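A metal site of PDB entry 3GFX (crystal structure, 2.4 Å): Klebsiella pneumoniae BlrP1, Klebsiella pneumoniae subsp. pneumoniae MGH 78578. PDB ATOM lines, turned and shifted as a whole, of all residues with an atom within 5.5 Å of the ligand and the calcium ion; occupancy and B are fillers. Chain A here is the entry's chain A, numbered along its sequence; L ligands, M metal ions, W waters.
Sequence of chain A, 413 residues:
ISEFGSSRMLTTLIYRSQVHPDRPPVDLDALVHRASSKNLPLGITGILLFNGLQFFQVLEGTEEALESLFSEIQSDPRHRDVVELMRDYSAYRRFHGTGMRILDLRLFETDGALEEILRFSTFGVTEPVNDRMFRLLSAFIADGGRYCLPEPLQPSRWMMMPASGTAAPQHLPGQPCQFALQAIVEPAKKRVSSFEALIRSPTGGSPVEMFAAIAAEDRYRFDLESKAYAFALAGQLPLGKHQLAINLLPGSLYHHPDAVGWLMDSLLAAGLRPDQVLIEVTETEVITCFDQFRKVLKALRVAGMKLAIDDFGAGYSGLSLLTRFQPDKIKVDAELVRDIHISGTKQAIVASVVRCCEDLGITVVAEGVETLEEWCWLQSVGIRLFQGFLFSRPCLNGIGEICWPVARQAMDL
O of Asn 247 sits at hydrogen-bond distance from N8 of the ligand. The guanidinium group of Arg 200 lies within salt-bridge range of an oxygen (O9) of the ligand, 2.8 Å away. An oxygen (O7) of the ligand lies within hydrogen-bond range of the backbone NH (N) of Phe 389 (2.8 Å). The side-chain carboxylate of Asp 223 lies within hydrogen-bond range of a nitrogen (N8) of the ligand (2.9 Å). N of Ile 199 is in hydrogen-bond range of N7 of the ligand, 2.9 Å away. A nitrogen (N3) of the ligand lies within hydrogen-bond range of the side-chain carboxylate (OE1) of Glu 370. NZ of Lys 227 is in hydrogen-bond range of O14 of the ligand (3.0 Å). NE2 of Gln 182 lies within hydrogen-bond range of N2 of the ligand.
The backbone carbonyl oxygen of Glu 280 sits at hydrogen-bond distance from the backbone NH of Leu 248, at 3.1 Å. The backbone carbonyl oxygen (O) of Gln 182 sits at hydrogen-bond distance from the backbone NH (N) of Glu 196 (2.8 Å). OE1 of Glu 196 lies within salt-bridge range of NZ of Lys 331, 3.3 Å away. The side-chain carboxylate (OE1) of Glu 196 lies within hydrogen-bond range of the side-chain amide nitrogen (NE2) of Gln 387. NZ of Lys 227 sits close to O of Asn 247 (3.3 Å). The side-chain amino group (NZ) of Lys 227 is in salt-bridge range of the side-chain carboxylate (OD1) of Asp 223 (2.8 Å). The side-chain amide oxygen (OE1) of Gln 182 sits at hydrogen-bond distance from the side-chain amide nitrogen (NE2) of Gln 387 (2.8 Å). N of Val 369 lies within hydrogen-bond range of O of Gln 387 (3.1 Å).
Merely in contact with the ligand: Phe 179 (3.9 Å), Leu 198 (3.4 Å), Pro 207 (3.3 Å), Phe 211 (3.8 Å), Leu 249 (3.96 Å), Asp 311 (3.6 Å), Gly 368 (3.5 Å), Val 369 (3.8 Å), Gly 388 (3.3 Å) and Pro 394 (3.4 Å). Hydrophobic or aromatic side chains that line the ligand: Phe 179, Leu 198, Ile 199, Pro 207, Phe 211, Leu 249, Phe 389 and Pro 394. Within 4 Å of the ligand: Phe 179, Gln 182, Glu 196, Leu 198, Ile 199, Arg 200, Pro 207, Phe 211, Asp 223, Lys 227, Asn 247, Leu 249, Asp 310, Asp 311, Gly 368, Val 369, Glu 370, Gly 388, Phe 389 and Pro 394. The nearest printed residue that does not touch the ligand is Ala 197 (4.0002 Å).
The calcium ion is bound by an oxygen (O1) of the ligand, the side-chain carboxylate of Asp 310, the side-chain carboxylate of Glu 280, the side-chain carboxylate of Glu 196, the side-chain amide oxygen of Asn 247 and water W9. The calcium ion has six donor atoms within binding distance.
Water W9 lies within hydrogen-bond range of the side-chain carboxylate of Glu 367, the side-chain carboxylate of Glu 196 and the side-chain amino group of Lys 331. Water W8 lies within hydrogen-bond range of O2 of the ligand (2.7 Å) and OD2 of Asp 311 (3.2 Å). Water W2 lies within hydrogen-bond range of the backbone NH (N) of Gly 368, a nitrogen (N2) of the ligand and the backbone carbonyl oxygen (O) of Gln 387. Water W7 lies within hydrogen-bond range of OE1 of Glu 370 (2.8 Å) and N4 of the ligand (3.1 Å). Water W6 lies within hydrogen-bond range of the backbone carbonyl oxygen (O) of Ala 197, the backbone NH (N) of Asn 247 and an oxygen (O14) of the ligand.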
ATOM      1  N   PHE A 179      16.262 -14.186  -8.909  1.00  0.00           N
ATOM      2  CA  PHE A 179      15.778 -13.621  -7.655  1.00  0.00           C
ATOM      3  C   PHE A 179      14.439 -12.909  -7.839  1.00  0.00           C
ATOM      4  O   PHE A 179      14.271 -12.110  -8.761  1.00  0.00           O
ATOM      5  CB  PHE A 179      16.800 -12.664  -7.047  1.00  0.00           C
ATOM      6  CG  PHE A 179      17.929 -13.360  -6.333  1.00  0.00           C
ATOM      7  CD1 PHE A 179      19.082 -13.710  -7.014  1.00  0.00           C
ATOM      8  CD2 PHE A 179      17.822 -13.664  -4.987  1.00  0.00           C
ATOM      9  CE1 PHE A 179      20.116 -14.356  -6.359  1.00  0.00           C
ATOM     10  CE2 PHE A 179      18.862 -14.312  -4.319  1.00  0.00           C
ATOM     11  CZ  PHE A 179      20.004 -14.648  -5.018  1.00  0.00           C
ATOM     12  N   GLN A 182      10.474  -8.723  -3.250  1.00  0.00           N
ATOM     13  CA  GLN A 182       9.300  -8.306  -2.495  1.00  0.00           C
ATOM     14  C   GLN A 182       9.607  -7.052  -1.688  1.00  0.00           C
ATOM     15  O   GLN A 182      10.625  -6.980  -0.994  1.00  0.00           O
ATOM     16  CB  GLN A 182       8.801  -9.423  -1.570  1.00  0.00           C
ATOM     17  CG  GLN A 182       7.418  -9.161  -0.982  1.00  0.00           C
ATOM     18  CD  GLN A 182       6.966 -10.232  -0.012  1.00  0.00           C
ATOM     19  OE1 GLN A 182       7.783 -10.933   0.578  1.00  0.00           O
ATOM     20  NE2 GLN A 182       5.658 -10.345   0.162  1.00  0.00           N
ATOM     21  N   GLU A 196      13.395  -7.166  -0.574  1.00  0.00           N
ATOM     22  CA  GLU A 196      14.053  -8.414  -0.185  1.00  0.00           C
ATOM     23  C   GLU A 196      14.224  -9.334  -1.385  1.00  0.00           C
ATOM     24  O   GLU A 196      13.284  -9.595  -2.131  1.00  0.00           O
ATOM     25  CB  GLU A 196      13.272  -9.129   0.924  1.00  0.00           C
ATOM     26  CG  GLU A 196      14.034 -10.324   1.504  1.00  0.00           C
ATOM     27  CD  GLU A 196      13.174 -11.219   2.379  1.00  0.00           C
ATOM     28  OE1 GLU A 196      11.988 -10.898   2.607  1.00  0.00           O
ATOM     29  OE2 GLU A 196      13.700 -12.245   2.857  1.00  0.00           O
ATOM     30  N   ALA A 197      15.451  -9.828  -1.559  1.00  0.00           N
ATOM     31  CA  ALA A 197      15.778 -10.743  -2.643  1.00  0.00           C
ATOM     32  C   ALA A 197      15.519 -12.196  -2.246  1.00  0.00           C
ATOM     33  O   ALA A 197      16.116 -12.711  -1.292  1.00  0.00           O
ATOM     34  CB  ALA A 197      17.231 -10.560  -3.064  1.00  0.00           C
ATOM     35  N   LEU A 198      14.605 -12.844  -2.963  1.00  0.00           N
ATOM     36  CA  LEU A 198      14.229 -14.218  -2.698  1.00  0.00           C
ATOM     37  C   LEU A 198      14.631 -15.093  -3.876  1.00  0.00           C
ATOM     38  O   LEU A 198      14.162 -14.893  -4.994  1.00  0.00           O
ATOM     39  CB  LEU A 198      12.718 -14.324  -2.462  1.00  0.00           C
ATOM     40  CG  LEU A 198      12.155 -13.469  -1.322  1.00  0.00           C
ATOM     41  CD1 LEU A 198      10.655 -13.255  -1.491  1.00  0.00           C
ATOM     42  CD2 LEU A 198      12.472 -14.068   0.044  1.00  0.00           C
ATOM     43  N   ILE A 199      15.499 -16.072  -3.631  1.00  0.00           N
ATOM     44  CA  ILE A 199      16.107 -16.864  -4.699  1.00  0.00           C
ATOM     45  C   ILE A 199      15.096 -17.758  -5.437  1.00  0.00           C
ATOM     46  O   ILE A 199      14.134 -18.255  -4.841  1.00  0.00           O
ATOM     47  CB  ILE A 199      17.334 -17.688  -4.177  1.00  0.00           C
ATOM     48  CG1 ILE A 199      18.295 -18.028  -5.331  1.00  0.00           C
ATOM     49  CG2 ILE A 199      16.911 -18.931  -3.398  1.00  0.00           C
ATOM     50  CD1 ILE A 199      19.619 -18.607  -4.880  1.00  0.00           C
ATOM     51  N   ARG A 200      15.303 -17.906  -6.712  1.00  0.00           N
ATOM     52  CA  ARG A 200      14.488 -18.771  -7.537  1.00  0.00           C
ATOM     53  C   ARG A 200      15.397 -19.626  -8.406  1.00  0.00           C
ATOM     54  O   ARG A 200      16.535 -19.239  -8.675  1.00  0.00           O
ATOM     55  CB  ARG A 200      13.524 -17.947  -8.410  1.00  0.00           C
ATOM     56  CG  ARG A 200      12.541 -17.058  -7.646  1.00  0.00           C
ATOM     57  CD  ARG A 200      11.396 -17.859  -7.057  1.00  0.00           C
ATOM     58  NE  ARG A 200      10.441 -17.035  -6.324  1.00  0.00           N
ATOM     59  CZ  ARG A 200      10.435 -16.877  -4.996  1.00  0.00           C
ATOM     60  NH1 ARG A 200      11.335 -17.499  -4.250  1.00  0.00           N
ATOM     61  NH2 ARG A 200       9.524 -16.095  -4.427  1.00  0.00           N
ATOM     62  N   SER A 206      10.929 -22.644  -6.344  1.00  0.00           N
ATOM     63  CA  SER A 206      11.141 -22.140  -4.982  1.00  0.00           C
ATOM     64  C   SER A 206      12.611 -22.218  -4.549  1.00  0.00           C
ATOM     65  O   SER A 206      13.417 -22.883  -5.205  1.00  0.00           O
ATOM     66  CB  SER A 206      10.248 -22.937  -4.026  1.00  0.00           C
ATOM     67  OG  SER A 206      10.614 -24.301  -3.999  1.00  0.00           O
ATOM     68  N   PRO A 207      12.973 -21.522  -3.442  1.00  0.00           N
ATOM     69  CA  PRO A 207      14.297 -21.691  -2.816  1.00  0.00           C
ATOM     70  C   PRO A 207      14.632 -23.138  -2.448  1.00  0.00           C
ATOM     71  O   PRO A 207      15.787 -23.528  -2.518  1.00  0.00           O
ATOM     72  CB  PRO A 207      14.190 -20.826  -1.554  1.00  0.00           C
ATOM     73  CG  PRO A 207      13.209 -19.786  -1.918  1.00  0.00           C
ATOM     74  CD  PRO A 207      12.183 -20.496  -2.734  1.00  0.00           C
ATOM     75  N   PHE A 211      17.948 -25.078  -4.020  1.00  0.00           N
ATOM     76  CA  PHE A 211      19.017 -25.677  -3.192  1.00  0.00           C
ATOM     77  C   PHE A 211      19.077 -27.209  -3.273  1.00  0.00           C
ATOM     78  O   PHE A 211      20.130 -27.796  -3.031  1.00  0.00           O
ATOM     79  CB  PHE A 211      18.917 -25.210  -1.736  1.00  0.00           C
ATOM     80  CG  PHE A 211      19.501 -23.841  -1.497  1.00  0.00           C
ATOM     81  CD1 PHE A 211      20.869 -23.673  -1.333  1.00  0.00           C
ATOM     82  CD2 PHE A 211      18.677 -22.712  -1.436  1.00  0.00           C
ATOM     83  CE1 PHE A 211      21.410 -22.410  -1.108  1.00  0.00           C
ATOM     84  CE2 PHE A 211      19.212 -21.454  -1.217  1.00  0.00           C
ATOM     85  CZ  PHE A 211      20.578 -21.303  -1.053  1.00  0.00           C
ATOM     86  N   ASP A 223      25.059 -20.402  -1.887  1.00  0.00           N
ATOM     87  CA  ASP A 223      24.266 -19.368  -1.200  1.00  0.00           C
ATOM     88  C   ASP A 223      24.985 -18.028  -1.197  1.00  0.00           C
ATOM     89  O   ASP A 223      24.380 -16.989  -1.439  1.00  0.00           O
ATOM     90  CB  ASP A 223      23.954 -19.822   0.228  1.00  0.00           C
ATOM     91  CG  ASP A 223      22.910 -18.959   0.907  1.00  0.00           C
ATOM     92  OD1 ASP A 223      22.206 -18.193   0.226  1.00  0.00           O
ATOM     93  OD2 ASP A 223      22.789 -19.049   2.146  1.00  0.00           O
ATOM     94  N   SER A 226      25.612 -16.859  -5.172  1.00  0.00           N
ATOM     95  CA  SER A 226      24.364 -16.479  -5.849  1.00  0.00           C
ATOM     96  C   SER A 226      24.008 -15.010  -5.653  1.00  0.00           C
ATOM     97  O   SER A 226      23.278 -14.422  -6.451  1.00  0.00           O
ATOM     98  CB  SER A 226      23.201 -17.343  -5.365  1.00  0.00           C
ATOM     99  OG  SER A 226      22.946 -17.144  -3.984  1.00  0.00           O
ATOM    100  N   LYS A 227      24.547 -14.424  -4.592  1.00  0.00           N
ATOM    101  CA  LYS A 227      24.231 -13.044  -4.197  1.00  0.00           C
ATOM    102  C   LYS A 227      24.733 -11.994  -5.173  1.00  0.00           C
ATOM    103  O   LYS A 227      24.236 -10.870  -5.185  1.00  0.00           O
ATOM    104  CB  LYS A 227      24.763 -12.758  -2.792  1.00  0.00           C
ATOM    105  CG  LYS A 227      24.125 -13.616  -1.711  1.00  0.00           C
ATOM    106  CD  LYS A 227      22.612 -13.511  -1.761  1.00  0.00           C
ATOM    107  CE  LYS A 227      21.952 -14.494  -0.833  1.00  0.00           C
ATOM    108  NZ  LYS A 227      21.961 -15.880  -1.338  1.00  0.00           N
ATOM    109  N   ASN A 247      19.096 -12.916   1.870  1.00  0.00           N
ATOM    110  CA  ASN A 247      19.055 -14.041   2.801  1.00  0.00           C
ATOM    111  C   ASN A 247      20.309 -14.890   2.719  1.00  0.00           C
ATOM    112  O   ASN A 247      20.660 -15.401   1.657  1.00  0.00           O
ATOM    113  CB  ASN A 247      17.838 -14.922   2.516  1.00  0.00           C
ATOM    114  CG  ASN A 247      16.535 -14.212   2.789  1.00  0.00           C
ATOM    115  OD1 ASN A 247      16.122 -14.094   3.943  1.00  0.00           O
ATOM    116  ND2 ASN A 247      15.869 -13.745   1.744  1.00  0.00           N
ATOM    117  N   LEU A 248      20.977 -15.066   3.861  1.00  0.00           N
ATOM    118  CA  LEU A 248      22.175 -15.906   3.915  1.00  0.00           C
ATOM    119  C   LEU A 248      22.151 -16.819   5.129  1.00  0.00           C
ATOM    120  O   LEU A 248      21.686 -16.433   6.209  1.00  0.00           O
ATOM    121  CB  LEU A 248      23.445 -15.051   3.935  1.00  0.00           C
ATOM    122  CG  LEU A 248      23.964 -14.508   2.609  1.00  0.00           C
ATOM    123  CD1 LEU A 248      25.012 -13.425   2.845  1.00  0.00           C
ATOM    124  CD2 LEU A 248      24.541 -15.632   1.739  1.00  0.00           C
ATOM    125  N   LEU A 249      22.641 -18.043   4.945  1.00  0.00           N
ATOM    126  CA  LEU A 249      22.935 -18.931   6.070  1.00  0.00           C
ATOM    127  C   LEU A 249      24.174 -18.384   6.769  1.00  0.00           C
ATOM    128  O   LEU A 249      25.106 -17.934   6.105  1.00  0.00           O
ATOM    129  CB  LEU A 249      23.183 -20.354   5.576  1.00  0.00           C
ATOM    130  CG  LEU A 249      21.982 -21.156   5.048  1.00  0.00           C
ATOM    131  CD1 LEU A 249      22.443 -22.280   4.139  1.00  0.00           C
ATOM    132  CD2 LEU A 249      21.133 -21.693   6.189  1.00  0.00           C
ATOM    133  N   GLU A 280      20.217 -10.899   6.030  1.00  0.00           N
ATOM    134  CA  GLU A 280      19.197 -11.562   6.818  1.00  0.00           C
ATOM    135  C   GLU A 280      19.612 -12.966   7.249  1.00  0.00           C
ATOM    136  O   GLU A 280      19.795 -13.852   6.412  1.00  0.00           O
ATOM    137  CB  GLU A 280      17.865 -11.602   6.080  1.00  0.00           C
ATOM    138  CG  GLU A 280      17.040 -10.337   6.220  1.00  0.00           C
ATOM    139  CD  GLU A 280      15.693 -10.442   5.543  1.00  0.00           C
ATOM    140  OE1 GLU A 280      15.234  -9.429   4.992  1.00  0.00           O
ATOM    141  OE2 GLU A 280      15.076 -11.537   5.573  1.00  0.00           O
ATOM    142  N   ASP A 310      15.970 -12.456  11.043  1.00  0.00           N
ATOM    143  CA  ASP A 310      14.731 -12.879  10.415  1.00  0.00           C
ATOM    144  C   ASP A 310      14.035 -13.947  11.244  1.00  0.00           C
ATOM    145  O   ASP A 310      14.686 -14.650  12.026  1.00  0.00           O
ATOM    146  CB  ASP A 310      15.016 -13.380   8.999  1.00  0.00           C
ATOM    147  CG  ASP A 310      13.776 -13.409   8.136  1.00  0.00           C
ATOM    148  OD1 ASP A 310      12.801 -12.674   8.436  1.00  0.00           O
ATOM    149  OD2 ASP A 310      13.767 -14.156   7.132  1.00  0.00           O
ATOM    150  N   ASP A 311      12.717 -14.066  11.063  1.00  0.00           N
ATOM    151  CA  ASP A 311      11.865 -15.002  11.818  1.00  0.00           C
ATOM    152  C   ASP A 311      12.037 -14.860  13.327  1.00  0.00           C
ATOM    153  O   ASP A 311      12.132 -15.853  14.057  1.00  0.00           O
ATOM    154  CB  ASP A 311      12.110 -16.456  11.377  1.00  0.00           C
ATOM    155  CG  ASP A 311      11.756 -16.701   9.915  1.00  0.00           C
ATOM    156  OD1 ASP A 311      10.759 -16.136   9.437  1.00  0.00           O
ATOM    157  OD2 ASP A 311      12.481 -17.476   9.258  1.00  0.00           O
ATOM    158  N   LYS A 331      12.828  -8.923  12.102  1.00  0.00           N
ATOM    159  CA  LYS A 331      11.623  -9.192  11.343  1.00  0.00           C
ATOM    160  C   LYS A 331      10.764 -10.203  12.102  1.00  0.00           C
ATOM    161  O   LYS A 331      11.122 -11.383  12.193  1.00  0.00           O
ATOM    162  CB  LYS A 331      11.964  -9.698   9.936  1.00  0.00           C
ATOM    163  CG  LYS A 331      12.999  -8.824   9.212  1.00  0.00           C
ATOM    164  CD  LYS A 331      13.305  -9.351   7.832  1.00  0.00           C
ATOM    165  CE  LYS A 331      12.490  -8.646   6.772  1.00  0.00           C
ATOM    166  NZ  LYS A 331      12.495  -9.392   5.490  1.00  0.00           N
ATOM    167  N   GLU A 367       6.243  -9.668   9.327  1.00  0.00           N
ATOM    168  CA  GLU A 367       6.264 -10.609   8.206  1.00  0.00           C
ATOM    169  C   GLU A 367       4.906 -11.237   7.957  1.00  0.00           C
ATOM    170  O   GLU A 367       4.115 -11.404   8.884  1.00  0.00           O
ATOM    171  CB  GLU A 367       7.257 -11.738   8.490  1.00  0.00           C
ATOM    172  CG  GLU A 367       8.702 -11.320   8.622  1.00  0.00           C
ATOM    173  CD  GLU A 367       9.390 -11.254   7.286  1.00  0.00           C
ATOM    174  OE1 GLU A 367       9.582 -12.318   6.660  1.00  0.00           O
ATOM    175  OE2 GLU A 367       9.725 -10.136   6.865  1.00  0.00           O
ATOM    176  N   GLY A 368       4.658 -11.617   6.709  1.00  0.00           N
ATOM    177  CA  GLY A 368       3.477 -12.399   6.342  1.00  0.00           C
ATOM    178  C   GLY A 368       2.142 -11.726   6.616  1.00  0.00           C
ATOM    179  O   GLY A 368       1.178 -12.376   7.004  1.00  0.00           O
ATOM    180  N   VAL A 369       2.102 -10.409   6.407  1.00  0.00           N
ATOM    181  CA  VAL A 369       0.887  -9.627   6.614  1.00  0.00           C
ATOM    182  C   VAL A 369      -0.060  -9.833   5.435  1.00  0.00           C
ATOM    183  O   VAL A 369       0.189  -9.348   4.337  1.00  0.00           O
ATOM    184  CB  VAL A 369       1.210  -8.130   6.803  1.00  0.00           C
ATOM    185  CG1 VAL A 369      -0.019  -7.379   7.316  1.00  0.00           C
ATOM    186  CG2 VAL A 369       2.386  -7.943   7.749  1.00  0.00           C
ATOM    187  N   GLU A 370      -1.138 -10.570   5.677  1.00  0.00           N
ATOM    188  CA  GLU A 370      -2.052 -10.993   4.620  1.00  0.00           C
ATOM    189  C   GLU A 370      -3.386 -10.249   4.603  1.00  0.00           C
ATOM    190  O   GLU A 370      -4.032 -10.143   3.553  1.00  0.00           O
ATOM    191  CB  GLU A 370      -2.311 -12.496   4.709  1.00  0.00           C
ATOM    192  CG  GLU A 370      -1.085 -13.376   4.468  1.00  0.00           C
ATOM    193  CD  GLU A 370      -1.411 -14.859   4.493  1.00  0.00           C
ATOM    194  OE1 GLU A 370      -0.731 -15.634   3.801  1.00  0.00           O
ATOM    195  OE2 GLU A 370      -2.361 -15.258   5.206  1.00  0.00           O
ATOM    196  N   GLN A 387       5.643  -6.314   5.588  1.00  0.00           N
ATOM    197  CA  GLN A 387       5.940  -7.171   4.451  1.00  0.00           C
ATOM    198  C   GLN A 387       4.894  -8.285   4.371  1.00  0.00           C
ATOM    199  O   GLN A 387       4.658  -8.985   5.356  1.00  0.00           O
ATOM    200  CB  GLN A 387       7.335  -7.769   4.570  1.00  0.00           C
ATOM    201  CG  GLN A 387       7.813  -8.484   3.314  1.00  0.00           C
ATOM    202  CD  GLN A 387       9.177  -9.121   3.471  1.00  0.00           C
ATOM    203  OE1 GLN A 387       9.953  -8.755   4.364  1.00  0.00           O
ATOM    204  NE2 GLN A 387       9.493 -10.086   2.615  1.00  0.00           N
ATOM    205  N   GLY A 388       4.295  -8.443   3.191  1.00  0.00           N
ATOM    206  CA  GLY A 388       3.280  -9.467   3.007  1.00  0.00           C
ATOM    207  C   GLY A 388       2.487  -9.326   1.720  1.00  0.00           C
ATOM    208  O   GLY A 388       2.589  -8.305   1.031  1.00  0.00           O
ATOM    209  N   PHE A 389       1.686 -10.344   1.409  1.00  0.00           N
ATOM    210  CA  PHE A 389       0.917 -10.411   0.172  1.00  0.00           C
ATOM    211  C   PHE A 389      -0.179  -9.345   0.060  1.00  0.00           C
ATOM    212  O   PHE A 389      -0.668  -9.080  -1.038  1.00  0.00           O
ATOM    213  CB  PHE A 389       0.284 -11.808   0.003  1.00  0.00           C
ATOM    214  CG  PHE A 389       1.270 -12.904  -0.292  1.00  0.00           C
ATOM    215  CD1 PHE A 389       2.529 -12.638  -0.807  1.00  0.00           C
ATOM    216  CD2 PHE A 389       0.918 -14.243  -0.071  1.00  0.00           C
ATOM    217  CE1 PHE A 389       3.438 -13.660  -1.074  1.00  0.00           C
ATOM    218  CE2 PHE A 389       1.806 -15.269  -0.346  1.00  0.00           C
ATOM    219  CZ  PHE A 389       3.065 -14.980  -0.843  1.00  0.00           C
ATOM    220  N   LEU A 390      -0.533  -8.743   1.191  1.00  0.00           N
ATOM    221  CA  LEU A 390      -1.523  -7.664   1.228  1.00  0.00           C
ATOM    222  C   LEU A 390      -1.032  -6.432   0.467  1.00  0.00           C
ATOM    223  O   LEU A 390      -1.816  -5.758  -0.213  1.00  0.00           O
ATOM    224  CB  LEU A 390      -1.846  -7.289   2.679  1.00  0.00           C
ATOM    225  CG  LEU A 390      -2.963  -6.279   2.941  1.00  0.00           C
ATOM    226  CD1 LEU A 390      -4.337  -6.882   2.669  1.00  0.00           C
ATOM    227  CD2 LEU A 390      -2.881  -5.750   4.371  1.00  0.00           C
ATOM    228  N   SER A 392       2.458  -6.272  -1.290  1.00  0.00           N
ATOM    229  CA  SER A 392       3.311  -6.588  -2.422  1.00  0.00           C
ATOM    230  C   SER A 392       3.652  -8.079  -2.486  1.00  0.00           C
ATOM    231  O   SER A 392       4.086  -8.670  -1.498  1.00  0.00           O
ATOM    232  CB  SER A 392       4.601  -5.766  -2.359  1.00  0.00           C
ATOM    233  OG  SER A 392       5.473  -6.074  -3.431  1.00  0.00           O
ATOM    234  N   PRO A 394       6.010 -11.125  -4.330  1.00  0.00           N
ATOM    235  CA  PRO A 394       7.336 -11.248  -4.938  1.00  0.00           C
ATOM    236  C   PRO A 394       7.288 -11.224  -6.459  1.00  0.00           C
ATOM    237  O   PRO A 394       6.440 -11.889  -7.059  1.00  0.00           O
ATOM    238  CB  PRO A 394       7.829 -12.615  -4.436  1.00  0.00           C
ATOM    239  CG  PRO A 394       7.068 -12.862  -3.192  1.00  0.00           C
ATOM    240  CD  PRO A 394       5.715 -12.262  -3.440  1.00  0.00           C
HETATM  241  P1  LIG L   1      11.619 -15.840   4.401  1.00  0.00           P
HETATM  242  O1  LIG L   1      12.687 -14.914   3.866  1.00  0.00           O
HETATM  243  O2  LIG L   1      11.527 -16.042   5.893  1.00  0.00           O
HETATM  244  O3  LIG L   1      10.187 -15.271   3.945  1.00  0.00           O
HETATM  245  C1  LIG L   1       9.871 -14.968   2.594  1.00  0.00           C
HETATM  246  C2  LIG L   1       8.923 -16.032   2.048  1.00  0.00           C
HETATM  247  O4  LIG L   1       7.612 -15.844   2.595  1.00  0.00           O
HETATM  248  C3  LIG L   1       8.780 -15.904   0.549  1.00  0.00           C
HETATM  249  O5  LIG L   1       8.701 -17.193  -0.029  1.00  0.00           O
HETATM  250  C4  LIG L   1       7.454 -15.252   0.385  1.00  0.00           C
HETATM  251  O6  LIG L   1       6.847 -15.270  -0.803  1.00  0.00           O
HETATM  252  C5  LIG L   1       6.759 -15.349   1.517  1.00  0.00           C
HETATM  253  N1  LIG L   1       5.781 -14.452   1.839  1.00  0.00           N
HETATM  254  C6  LIG L   1       5.934 -13.184   1.750  1.00  0.00           C
HETATM  255  N2  LIG L   1       4.838 -12.628   2.129  1.00  0.00           N
HETATM  256  C7  LIG L   1       3.931 -13.571   2.494  1.00  0.00           C
HETATM  257  C8  LIG L   1       2.623 -13.553   2.974  1.00  0.00           C
HETATM  258  O7  LIG L   1       2.017 -12.482   3.167  1.00  0.00           O
HETATM  259  N3  LIG L   1       2.013 -14.729   3.238  1.00  0.00           N
HETATM  260  C9  LIG L   1       2.647 -15.906   3.033  1.00  0.00           C
HETATM  261  N4  LIG L   1       1.986 -17.056   3.319  1.00  0.00           N
HETATM  262  N5  LIG L   1       3.923 -15.950   2.564  1.00  0.00           N
HETATM  263  C10 LIG L   1       4.568 -14.794   2.292  1.00  0.00           C
HETATM  264  P2  LIG L   1       9.998 -17.941  -0.614  1.00  0.00           P
HETATM  265  O8  LIG L   1       9.417 -19.090  -1.582  1.00  0.00           O
HETATM  266  O9  LIG L   1      10.763 -16.923  -1.595  1.00  0.00           O
HETATM  267  O10 LIG L   1      11.105 -18.221   0.519  1.00  0.00           O
HETATM  268  C11 LIG L   1      11.226 -19.446   1.229  1.00  0.00           C
HETATM  269  C12 LIG L   1      12.397 -19.054   2.139  1.00  0.00           C
HETATM  270  O11 LIG L   1      13.645 -19.325   1.488  1.00  0.00           O
HETATM  271  C13 LIG L   1      12.457 -17.575   2.526  1.00  0.00           C
HETATM  272  O12 LIG L   1      11.741 -17.297   3.725  1.00  0.00           O
HETATM  273  C14 LIG L   1      13.935 -17.315   2.633  1.00  0.00           C
HETATM  274  O13 LIG L   1      14.387 -17.800   3.797  1.00  0.00           O
HETATM  275  C15 LIG L   1      14.374 -18.086   1.647  1.00  0.00           C
HETATM  276  N6  LIG L   1      15.348 -17.665   0.790  1.00  0.00           N
HETATM  277  C16 LIG L   1      15.039 -16.924  -0.272  1.00  0.00           C
HETATM  278  N7  LIG L   1      16.231 -16.688  -0.877  1.00  0.00           N
HETATM  279  C17 LIG L   1      17.218 -17.287  -0.170  1.00  0.00           C
HETATM  280  C18 LIG L   1      18.602 -17.365  -0.334  1.00  0.00           C
HETATM  281  O14 LIG L   1      19.146 -16.801  -1.303  1.00  0.00           O
HETATM  282  N8  LIG L   1      19.329 -18.057   0.564  1.00  0.00           N
HETATM  283  C19 LIG L   1      18.752 -18.669   1.618  1.00  0.00           C
HETATM  284  N9  LIG L   1      19.532 -19.358   2.504  1.00  0.00           N
HETATM  285  N10 LIG L   1      17.406 -18.612   1.812  1.00  0.00           N
HETATM  286  C20 LIG L   1      16.647 -17.931   0.925  1.00  0.00           C
HETATM  287 CA    CA M   1      13.942 -13.491   4.900  1.00  0.00          CA
HETATM  288  O   HOH W   1       3.204 -16.532   6.165  1.00  0.00           O
HETATM  289  O   HOH W   2       6.338 -11.841   4.561  1.00  0.00           O
HETATM  290  O   HOH W   3       8.367 -20.015  -3.559  1.00  0.00           O
HETATM  291  O   HOH W   4       6.090 -17.560  -1.639  1.00  0.00           O
HETATM  292  O   HOH W   5       5.852 -15.007   5.276  1.00  0.00           O
HETATM  293  O   HOH W   6      18.434 -13.778  -0.767  1.00  0.00           O
HETATM  294  O   HOH W   7      -0.614 -18.369   4.433  1.00  0.00           O
HETATM  295  O   HOH W   8      13.959 -17.033   6.464  1.00  0.00           O
HETATM  296  O   HOH W   9      11.677 -12.153   5.058  1.00  0.00           O
